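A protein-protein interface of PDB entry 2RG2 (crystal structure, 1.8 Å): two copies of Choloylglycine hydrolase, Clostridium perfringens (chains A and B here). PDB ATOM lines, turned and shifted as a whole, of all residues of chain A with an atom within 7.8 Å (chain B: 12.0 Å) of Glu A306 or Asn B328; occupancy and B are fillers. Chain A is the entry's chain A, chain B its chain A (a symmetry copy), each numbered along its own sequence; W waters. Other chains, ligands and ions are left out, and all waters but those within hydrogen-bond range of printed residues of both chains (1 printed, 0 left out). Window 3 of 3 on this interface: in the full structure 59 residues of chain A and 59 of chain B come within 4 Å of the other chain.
No position is printed for both chains.
Water W1 lies within hydrogen-bond range of the backbone carbonyl oxygen (O) of Ala A300 (2.8 Å), the chain-end carboxylate (O) of Asn B328 (2.9 Å) and the backbone NH (N) of Val B327 (3.4 Å).
Among the printed residues, merely in contact across the chains: Lys A305 with Asn B328, Ile A301 with Asn B328, Ile A301 with Val B327, Ala A300 with His B326, Asn A299 with Val B327, Ala A300 with Ile B324, Tyr A316 with Asn B328 and Ala A300 with Asn B328.
The side-chain carboxylate (OE2) of Glu A306 is in hydrogen-bond range of the side-chain amide nitrogen (ND2) of Asn B328 (3.0 Å).
The backbone NH of Asp A302 lies within hydrogen-bond range of the side-chain amide oxygen of Asn B328, at 2.9 Å.
The side-chain amide nitrogen of Asn B325 lies within hydrogen-bond range of the side-chain amide oxygen of Asn A299 (3.0 Å).
N of Val B327 sits at hydrogen-bond distance from O of Ala A300, 2.8 Å away.
O of Asn B325 is in hydrogen-bond range of N of Ala A300.
Hydrophobic or aromatic side chains of chain B that line the printed part of chain A: Ile B324, His B326 and Val B327.
Of the 24 printed residues of chain A, 7 touch a printed residue of chain B.
Hydrophobic or aromatic side chains of chain A within 4 Å of the printed part of chain B: Ala A300, Ile A301 and Tyr A316.
Among the printed residues, no Asp or Glu carboxylate lies within 4 Å of a Lys or Arg side-chain nitrogen of the other chain.
The backbone NH (N) of Tyr A288 is in hydrogen-bond range of the backbone carbonyl oxygen (O) of Ile A301, at 2.8 Å.
The side-chain carboxylate (OE2) of Glu A306 lies within hydrogen-bond range of the side-chain hydroxyl (OH) of Tyr A316 (2.7 Å).
OD1 of Asp A302 is in hydrogen-bond range of N of Asn A304 (2.8 Å).
No residue of chain B comes within 4 Å of Phe A31.
Ile A287 touches none of the printed residues of chain B.
Tyr A288 touches none of the printed residues of chain B.
Of chain B, only Val B327 and Asn B328 come within 4 Å of Ile A301.
No residue of chain B comes within 4 Å of Asn A304.
Of chain B, only Asn B328 comes within 4 Å of Lys A305.
Of chain B, only Asn B328 comes within 4 Å of Glu A306.
No residue of chain B comes within 4 Å of Asn A307.
No residue of chain B comes within 4 Å of Leu A308.
No residue of chain B comes within 4 Å of Lys A314.
Printed residues of chain A within 4 Å of Ile B324: Ala A300.
Printed residues of chain A within 4 Å of Asn B325: Asn A299 (3.0 Å) and Ala A300 (2.8 Å).
Of the printed residues of chain A, His B326 touches Ala A300.
The nearest residue of chain B that does not touch Glu A306 is Val B327 (7.1 Å).
The nearest residue of chain A that does not touch Asn B328 is Met A303 (4.8 Å).
The nearest printed residue of chain A that does not touch Asn B325 is Ile A301 (5.6 Å).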
ATOM      1  N   PHE A  31     -21.391  10.010  -5.522  1.00  0.00           N
ATOM      2  CA  PHE A  31     -22.388  10.885  -4.931  1.00  0.00           C
ATOM      3  C   PHE A  31     -23.746  10.189  -4.970  1.00  0.00           C
ATOM      4  O   PHE A  31     -24.150   9.684  -6.024  1.00  0.00           O
ATOM      5  CB  PHE A  31     -22.485  12.204  -5.696  1.00  0.00           C
ATOM      6  CG  PHE A  31     -23.717  13.016  -5.349  1.00  0.00           C
ATOM      7  CD1 PHE A  31     -23.803  13.698  -4.144  1.00  0.00           C
ATOM      8  CD2 PHE A  31     -24.805  13.066  -6.227  1.00  0.00           C
ATOM      9  CE1 PHE A  31     -24.950  14.442  -3.813  1.00  0.00           C
ATOM     10  CE2 PHE A  31     -25.953  13.805  -5.905  1.00  0.00           C
ATOM     11  CZ  PHE A  31     -26.026  14.493  -4.696  1.00  0.00           C
ATOM     12  N   ILE A  32     -24.440  10.184  -3.831  1.00  0.00           N
ATOM     13  CA  ILE A  32     -25.795   9.649  -3.754  1.00  0.00           C
ATOM     14  C   ILE A  32     -26.721  10.750  -3.236  1.00  0.00           C
ATOM     15  O   ILE A  32     -26.526  11.263  -2.116  1.00  0.00           O
ATOM     16  CB  ILE A  32     -25.909   8.436  -2.801  1.00  0.00           C
ATOM     17  CG1 ILE A  32     -24.838   7.384  -3.091  1.00  0.00           C
ATOM     18  CG2 ILE A  32     -27.318   7.806  -2.905  1.00  0.00           C
ATOM     19  CD1 ILE A  32     -24.650   6.376  -1.961  1.00  0.00           C
ATOM     20  N   PRO A  33     -27.750  11.115  -4.033  1.00  0.00           N
ATOM     21  CA  PRO A  33     -28.719  12.096  -3.545  1.00  0.00           C
ATOM     22  C   PRO A  33     -29.495  11.569  -2.324  1.00  0.00           C
ATOM     23  O   PRO A  33     -29.421  10.377  -2.012  1.00  0.00           O
ATOM     24  CB  PRO A  33     -29.653  12.330  -4.747  1.00  0.00           C
ATOM     25  CG  PRO A  33     -29.344  11.257  -5.733  1.00  0.00           C
ATOM     26  CD  PRO A  33     -28.020  10.653  -5.411  1.00  0.00           C
ATOM     27  N   ALA A  52     -28.002  12.990   1.707  1.00  0.00           N
ATOM     28  CA  ALA A  52     -27.103  12.877   0.546  1.00  0.00           C
ATOM     29  C   ALA A  52     -25.687  12.543   1.028  1.00  0.00           C
ATOM     30  O   ALA A  52     -25.263  13.028   2.089  1.00  0.00           O
ATOM     31  CB  ALA A  52     -27.109  14.170  -0.254  1.00  0.00           C
ATOM     32  N   LEU A  54     -21.411  11.667  -0.067  1.00  0.00           N
ATOM     33  CA  LEU A  54     -20.334  11.853  -1.041  1.00  0.00           C
ATOM     34  C   LEU A  54     -19.061  11.244  -0.482  1.00  0.00           C
ATOM     35  O   LEU A  54     -18.697  11.551   0.653  1.00  0.00           O
ATOM     36  CB  LEU A  54     -20.126  13.347  -1.330  1.00  0.00           C
ATOM     37  CG  LEU A  54     -18.936  13.745  -2.236  1.00  0.00           C
ATOM     38  CD1 LEU A  54     -19.123  13.135  -3.620  1.00  0.00           C
ATOM     39  CD2 LEU A  54     -18.818  15.267  -2.304  1.00  0.00           C
ATOM     40  N   GLY A 286     -19.595  20.442   2.655  1.00  0.00           N
ATOM     41  CA  GLY A 286     -19.951  19.324   1.757  1.00  0.00           C
ATOM     42  C   GLY A 286     -18.970  19.150   0.597  1.00  0.00           C
ATOM     43  O   GLY A 286     -19.336  18.678  -0.485  1.00  0.00           O
ATOM     44  N   ILE A 287     -17.725  19.557   0.824  1.00  0.00           N
ATOM     45  CA  ILE A 287     -16.681  19.393  -0.173  1.00  0.00           C
ATOM     46  C   ILE A 287     -15.757  18.243   0.206  1.00  0.00           C
ATOM     47  O   ILE A 287     -15.198  18.218   1.317  1.00  0.00           O
ATOM     48  CB  ILE A 287     -15.848  20.686  -0.360  1.00  0.00           C
ATOM     49  CG1 ILE A 287     -16.779  21.860  -0.712  1.00  0.00           C
ATOM     50  CG2 ILE A 287     -14.792  20.440  -1.477  1.00  0.00           C
ATOM     51  CD1 ILE A 287     -16.133  23.239  -0.675  1.00  0.00           C
ATOM     52  N   TYR A 288     -15.624  17.297  -0.724  1.00  0.00           N
ATOM     53  CA  TYR A 288     -14.694  16.183  -0.612  1.00  0.00           C
ATOM     54  C   TYR A 288     -13.438  16.570  -1.402  1.00  0.00           C
ATOM     55  O   TYR A 288     -13.479  16.680  -2.635  1.00  0.00           O
ATOM     56  CB  TYR A 288     -15.332  14.898  -1.188  1.00  0.00           C
ATOM     57  CG  TYR A 288     -14.520  13.633  -0.981  1.00  0.00           C
ATOM     58  CD1 TYR A 288     -13.518  13.267  -1.884  1.00  0.00           C
ATOM     59  CD2 TYR A 288     -14.762  12.787   0.115  1.00  0.00           C
ATOM     60  CE1 TYR A 288     -12.772  12.102  -1.716  1.00  0.00           C
ATOM     61  CE2 TYR A 288     -14.003  11.646   0.315  1.00  0.00           C
ATOM     62  CZ  TYR A 288     -13.007  11.305  -0.609  1.00  0.00           C
ATOM     63  OH  TYR A 288     -12.250  10.179  -0.453  1.00  0.00           O
ATOM     64  N   ASN A 299      -8.020  17.918  -5.626  1.00  0.00           N
ATOM     65  CA  ASN A 299      -9.242  17.979  -6.411  1.00  0.00           C
ATOM     66  C   ASN A 299     -10.400  18.135  -5.462  1.00  0.00           C
ATOM     67  O   ASN A 299     -10.370  17.570  -4.355  1.00  0.00           O
ATOM     68  CB  ASN A 299      -9.410  16.668  -7.182  1.00  0.00           C
ATOM     69  CG  ASN A 299      -8.186  16.320  -7.982  1.00  0.00           C
ATOM     70  OD1 ASN A 299      -7.950  16.893  -9.042  1.00  0.00           O
ATOM     71  ND2 ASN A 299      -7.385  15.376  -7.472  1.00  0.00           N
ATOM     72  N   ALA A 300     -11.416  18.888  -5.883  1.00  0.00           N
ATOM     73  CA  ALA A 300     -12.565  19.185  -5.025  1.00  0.00           C
ATOM     74  C   ALA A 300     -13.839  18.759  -5.706  1.00  0.00           C
ATOM     75  O   ALA A 300     -14.107  19.194  -6.832  1.00  0.00           O
ATOM     76  CB  ALA A 300     -12.640  20.686  -4.716  1.00  0.00           C
ATOM     77  N   ILE A 301     -14.621  17.923  -5.014  1.00  0.00           N
ATOM     78  CA  ILE A 301     -16.000  17.618  -5.432  1.00  0.00           C
ATOM     79  C   ILE A 301     -16.929  18.179  -4.363  1.00  0.00           C
ATOM     80  O   ILE A 301     -16.817  17.823  -3.183  1.00  0.00           O
ATOM     81  CB  ILE A 301     -16.256  16.112  -5.674  1.00  0.00           C
ATOM     82  CG1 ILE A 301     -15.386  15.580  -6.818  1.00  0.00           C
ATOM     83  CG2 ILE A 301     -17.733  15.870  -6.018  1.00  0.00           C
ATOM     84  CD1 ILE A 301     -14.182  14.816  -6.379  1.00  0.00           C
ATOM     85  N   ASP A 302     -17.816  19.081  -4.781  1.00  0.00           N
ATOM     86  CA  ASP A 302     -18.723  19.779  -3.864  1.00  0.00           C
ATOM     87  C   ASP A 302     -20.130  19.209  -4.044  1.00  0.00           C
ATOM     88  O   ASP A 302     -20.749  19.412  -5.093  1.00  0.00           O
ATOM     89  CB  ASP A 302     -18.694  21.285  -4.157  1.00  0.00           C
ATOM     90  CG  ASP A 302     -19.546  22.112  -3.194  1.00  0.00           C
ATOM     91  OD1 ASP A 302     -20.404  21.563  -2.473  1.00  0.00           O
ATOM     92  OD2 ASP A 302     -19.353  23.344  -3.167  1.00  0.00           O
ATOM     93  N   MET A 303     -20.637  18.495  -3.038  1.00  0.00           N
ATOM     94  CA  MET A 303     -21.960  17.872  -3.181  1.00  0.00           C
ATOM     95  C   MET A 303     -23.054  18.915  -3.377  1.00  0.00           C
ATOM     96  O   MET A 303     -24.105  18.623  -3.960  1.00  0.00           O
ATOM     97  CB  MET A 303     -22.305  16.944  -2.000  1.00  0.00           C
ATOM     98  CG  MET A 303     -22.761  17.676  -0.759  1.00  0.00           C
ATOM     99  SD  MET A 303     -23.393  16.540   0.477  1.00  0.00           S
ATOM    100  CE  MET A 303     -21.910  15.823   1.080  1.00  0.00           C
ATOM    101  N   ASN A 304     -22.804  20.132  -2.911  1.00  0.00           N
ATOM    102  CA  ASN A 304     -23.795  21.197  -3.041  1.00  0.00           C
ATOM    103  C   ASN A 304     -23.908  21.771  -4.449  1.00  0.00           C
ATOM    104  O   ASN A 304     -24.803  22.570  -4.734  1.00  0.00           O
ATOM    105  CB  ASN A 304     -23.553  22.277  -1.990  1.00  0.00           C
ATOM    106  CG  ASN A 304     -23.789  21.763  -0.599  1.00  0.00           C
ATOM    107  OD1 ASN A 304     -24.913  21.358  -0.252  1.00  0.00           O
ATOM    108  ND2 ASN A 304     -22.727  21.721   0.207  1.00  0.00           N
ATOM    109  N   LYS A 305     -23.012  21.347  -5.334  1.00  0.00           N
ATOM    110  CA  LYS A 305     -23.123  21.684  -6.750  1.00  0.00           C
ATOM    111  C   LYS A 305     -24.040  20.683  -7.465  1.00  0.00           C
ATOM    112  O   LYS A 305     -24.400  20.882  -8.635  1.00  0.00           O
ATOM    113  CB  LYS A 305     -21.739  21.752  -7.396  1.00  0.00           C
ATOM    114  CG  LYS A 305     -20.976  23.006  -6.971  1.00  0.00           C
ATOM    115  CD  LYS A 305     -19.612  23.021  -7.584  1.00  0.00           C
ATOM    116  CE  LYS A 305     -18.719  24.058  -6.952  1.00  0.00           C
ATOM    117  NZ  LYS A 305     -19.170  25.453  -7.253  1.00  0.00           N
ATOM    118  N   GLU A 306     -24.435  19.624  -6.759  1.00  0.00           N
ATOM    119  CA  GLU A 306     -25.372  18.643  -7.294  1.00  0.00           C
ATOM    120  C   GLU A 306     -26.806  18.924  -6.810  1.00  0.00           C
ATOM    121  O   GLU A 306     -27.022  19.699  -5.881  1.00  0.00           O
ATOM    122  CB  GLU A 306     -24.951  17.213  -6.925  1.00  0.00           C
ATOM    123  CG  GLU A 306     -23.511  16.817  -7.357  1.00  0.00           C
ATOM    124  CD  GLU A 306     -23.252  16.897  -8.875  1.00  0.00           C
ATOM    125  OE1 GLU A 306     -24.214  16.881  -9.668  1.00  0.00           O
ATOM    126  OE2 GLU A 306     -22.066  16.964  -9.291  1.00  0.00           O
ATOM    127  N   ASN A 307     -27.778  18.320  -7.483  1.00  0.00           N
ATOM    128  CA  ASN A 307     -29.155  18.347  -6.997  1.00  0.00           C
ATOM    129  C   ASN A 307     -29.268  17.288  -5.901  1.00  0.00           C
ATOM    130  O   ASN A 307     -29.216  16.089  -6.177  1.00  0.00           O
ATOM    131  CB  ASN A 307     -30.120  18.066  -8.159  1.00  0.00           C
ATOM    132  CG  ASN A 307     -31.573  18.027  -7.727  1.00  0.00           C
ATOM    133  OD1 ASN A 307     -31.906  18.311  -6.579  1.00  0.00           O
ATOM    134  ND2 ASN A 307     -32.451  17.678  -8.665  1.00  0.00           N
ATOM    135  N   LEU A 308     -29.402  17.736  -4.654  1.00  0.00           N
ATOM    136  CA  LEU A 308     -29.461  16.809  -3.509  1.00  0.00           C
ATOM    137  C   LEU A 308     -30.735  15.959  -3.541  1.00  0.00           C
ATOM    138  O   LEU A 308     -30.811  14.893  -2.925  1.00  0.00           O
ATOM    139  CB  LEU A 308     -29.272  17.555  -2.179  1.00  0.00           C
ATOM    140  CG  LEU A 308     -27.960  18.347  -1.992  1.00  0.00           C
ATOM    141  CD1 LEU A 308     -27.847  18.909  -0.577  1.00  0.00           C
ATOM    142  CD2 LEU A 308     -26.733  17.488  -2.295  1.00  0.00           C
ATOM    143  N   ASP A 309     -31.714  16.426  -4.316  1.00  0.00           N
ATOM    144  CA  ASP A 309     -32.945  15.676  -4.571  1.00  0.00           C
ATOM    145  C   ASP A 309     -32.950  15.020  -5.936  1.00  0.00           C
ATOM    146  O   ASP A 309     -34.024  14.672  -6.460  1.00  0.00           O
ATOM    147  CB  ASP A 309     -34.142  16.612  -4.456  1.00  0.00           C
ATOM    148  CG  ASP A 309     -34.304  17.132  -3.073  1.00  0.00           C
ATOM    149  OD1 ASP A 309     -34.319  16.301  -2.140  1.00  0.00           O
ATOM    150  OD2 ASP A 309     -34.365  18.357  -2.913  1.00  0.00           O
ATOM    151  N   GLY A 310     -31.755  14.855  -6.511  1.00  0.00           N
ATOM    152  CA  GLY A 310     -31.587  14.146  -7.786  1.00  0.00           C
ATOM    153  C   GLY A 310     -32.029  12.689  -7.784  1.00  0.00           C
ATOM    154  O   GLY A 310     -32.266  12.087  -6.728  1.00  0.00           O
ATOM    155  N   GLU A 312     -30.301  10.134  -9.622  1.00  0.00           N
ATOM    156  CA  GLU A 312     -29.223   9.268 -10.078  1.00  0.00           C
ATOM    157  C   GLU A 312     -28.025   9.294  -9.132  1.00  0.00           C
ATOM    158  O   GLU A 312     -27.652  10.356  -8.661  1.00  0.00           O
ATOM    159  CB  GLU A 312     -28.724   9.742 -11.445  1.00  0.00           C
ATOM    160  CG  GLU A 312     -29.821   9.872 -12.530  1.00  0.00           C
ATOM    161  CD  GLU A 312     -29.269  10.270 -13.881  1.00  0.00           C
ATOM    162  OE1 GLU A 312     -28.242   9.700 -14.307  1.00  0.00           O
ATOM    163  OE2 GLU A 312     -29.882  11.137 -14.536  1.00  0.00           O
ATOM    164  N   LYS A 314     -24.161   9.518  -8.944  1.00  0.00           N
ATOM    165  CA  LYS A 314     -23.203  10.139  -9.852  1.00  0.00           C
ATOM    166  C   LYS A 314     -21.806   9.737  -9.426  1.00  0.00           C
ATOM    167  O   LYS A 314     -21.550   9.566  -8.234  1.00  0.00           O
ATOM    168  CB  LYS A 314     -23.334  11.658  -9.840  1.00  0.00           C
ATOM    169  CG  LYS A 314     -24.697  12.153 -10.388  1.00  0.00           C
ATOM    170  CD  LYS A 314     -24.801  13.651 -10.376  1.00  0.00           C
ATOM    171  CE  LYS A 314     -24.303  14.274 -11.674  1.00  0.00           C
ATOM    172  NZ  LYS A 314     -25.130  13.873 -12.854  1.00  0.00           N
ATOM    173  N   THR A 315     -20.913   9.573 -10.394  1.00  0.00           N
ATOM    174  CA  THR A 315     -19.525   9.234 -10.063  1.00  0.00           C
ATOM    175  C   THR A 315     -18.565  10.215 -10.729  1.00  0.00           C
ATOM    176  O   THR A 315     -18.924  10.928 -11.689  1.00  0.00           O
ATOM    177  CB  THR A 315     -19.149   7.777 -10.404  1.00  0.00           C
ATOM    178  OG1 THR A 315     -19.169   7.578 -11.830  1.00  0.00           O
ATOM    179  CG2 THR A 315     -20.088   6.781  -9.726  1.00  0.00           C
ATOM    180  N   TYR A 316     -17.358  10.291 -10.174  1.00  0.00           N
ATOM    181  CA  TYR A 316     -16.305  11.157 -10.695  1.00  0.00           C
ATOM    182  C   TYR A 316     -15.032  10.312 -10.753  1.00  0.00           C
ATOM    183  O   TYR A 316     -14.746   9.554  -9.830  1.00  0.00           O
ATOM    184  CB  TYR A 316     -16.128  12.412  -9.818  1.00  0.00           C
ATOM    185  CG  TYR A 316     -17.447  13.058  -9.379  1.00  0.00           C
ATOM    186  CD1 TYR A 316     -18.182  12.524  -8.310  1.00  0.00           C
ATOM    187  CD2 TYR A 316     -17.960  14.194 -10.026  1.00  0.00           C
ATOM    188  CE1 TYR A 316     -19.384  13.091  -7.894  1.00  0.00           C
ATOM    189  CE2 TYR A 316     -19.185  14.784  -9.598  1.00  0.00           C
ATOM    190  CZ  TYR A 316     -19.887  14.213  -8.536  1.00  0.00           C
ATOM    191  OH  TYR A 316     -21.096  14.739  -8.080  1.00  0.00           O
ATOM    192  N   ILE B 324      -6.391  24.539  -6.634  1.00  0.00           N
ATOM    193  CA  ILE B 324      -7.307  23.401  -6.523  1.00  0.00           C
ATOM    194  C   ILE B 324      -8.027  23.140  -7.847  1.00  0.00           C
ATOM    195  O   ILE B 324      -8.447  24.097  -8.513  1.00  0.00           O
ATOM    196  CB  ILE B 324      -8.342  23.683  -5.412  1.00  0.00           C
ATOM    197  CG1 ILE B 324      -7.640  23.702  -4.050  1.00  0.00           C
ATOM    198  CG2 ILE B 324      -9.472  22.641  -5.376  1.00  0.00           C
ATOM    199  CD1 ILE B 324      -8.400  24.453  -2.989  1.00  0.00           C
ATOM    200  N   ASN B 325      -8.124  21.865  -8.226  1.00  0.00           N
ATOM    201  CA  ASN B 325      -8.945  21.446  -9.360  1.00  0.00           C
ATOM    202  C   ASN B 325     -10.395  21.241  -8.910  1.00  0.00           C
ATOM    203  O   ASN B 325     -10.688  20.291  -8.214  1.00  0.00           O
ATOM    204  CB  ASN B 325      -8.418  20.155  -9.974  1.00  0.00           C
ATOM    205  CG  ASN B 325      -9.298  19.668 -11.098  1.00  0.00           C
ATOM    206  OD1 ASN B 325      -9.706  20.456 -11.954  1.00  0.00           O
ATOM    207  ND2 ASN B 325      -9.616  18.381 -11.096  1.00  0.00           N
ATOM    208  N   HIS B 326     -11.284  22.146  -9.297  1.00  0.00           N
ATOM    209  CA  HIS B 326     -12.695  22.016  -8.947  1.00  0.00           C
ATOM    210  C   HIS B 326     -13.398  21.108  -9.933  1.00  0.00           C
ATOM    211  O   HIS B 326     -13.721  21.517 -11.066  1.00  0.00           O
ATOM    212  CB  HIS B 326     -13.352  23.392  -8.866  1.00  0.00           C
ATOM    213  CG  HIS B 326     -12.794  24.234  -7.768  1.00  0.00           C
ATOM    214  ND1 HIS B 326     -13.243  24.153  -6.465  1.00  0.00           N
ATOM    215  CD2 HIS B 326     -11.781  25.129  -7.763  1.00  0.00           C
ATOM    216  CE1 HIS B 326     -12.544  24.989  -5.712  1.00  0.00           C
ATOM    217  NE2 HIS B 326     -11.662  25.600  -6.477  1.00  0.00           N
ATOM    218  N   VAL B 327     -13.622  19.872  -9.503  1.00  0.00           N
ATOM    219  CA  VAL B 327     -14.018  18.772 -10.404  1.00  0.00           C
ATOM    220  C   VAL B 327     -15.419  18.973 -10.974  1.00  0.00           C
ATOM    221  O   VAL B 327     -15.658  18.717 -12.166  1.00  0.00           O
ATOM    222  CB  VAL B 327     -13.932  17.386  -9.711  1.00  0.00           C
ATOM    223  CG1 VAL B 327     -14.450  16.263 -10.627  1.00  0.00           C
ATOM    224  CG2 VAL B 327     -12.495  17.090  -9.318  1.00  0.00           C
ATOM    225  N   ASN B 328     -16.327  19.416 -10.116  1.00  0.00           N
ATOM    226  CA  ASN B 328     -17.718  19.650 -10.511  1.00  0.00           C
ATOM    227  C   ASN B 328     -18.113  21.069 -10.182  1.00  0.00           C
ATOM    228  O   ASN B 328     -17.308  21.859  -9.632  1.00  0.00           O
ATOM    229  CB  ASN B 328     -18.652  18.631  -9.840  1.00  0.00           C
ATOM    230  CG  ASN B 328     -18.828  18.876  -8.344  1.00  0.00           C
ATOM    231  OD1 ASN B 328     -17.942  19.416  -7.675  1.00  0.00           O
ATOM    232  ND2 ASN B 328     -19.986  18.466  -7.809  1.00  0.00           N
ATOM    233  OXT ASN B 328     -19.255  21.473 -10.471  1.00  0.00           O
HETATM  234  O   HOH W   1     -15.714  21.473  -7.287  1.00  0.00           O
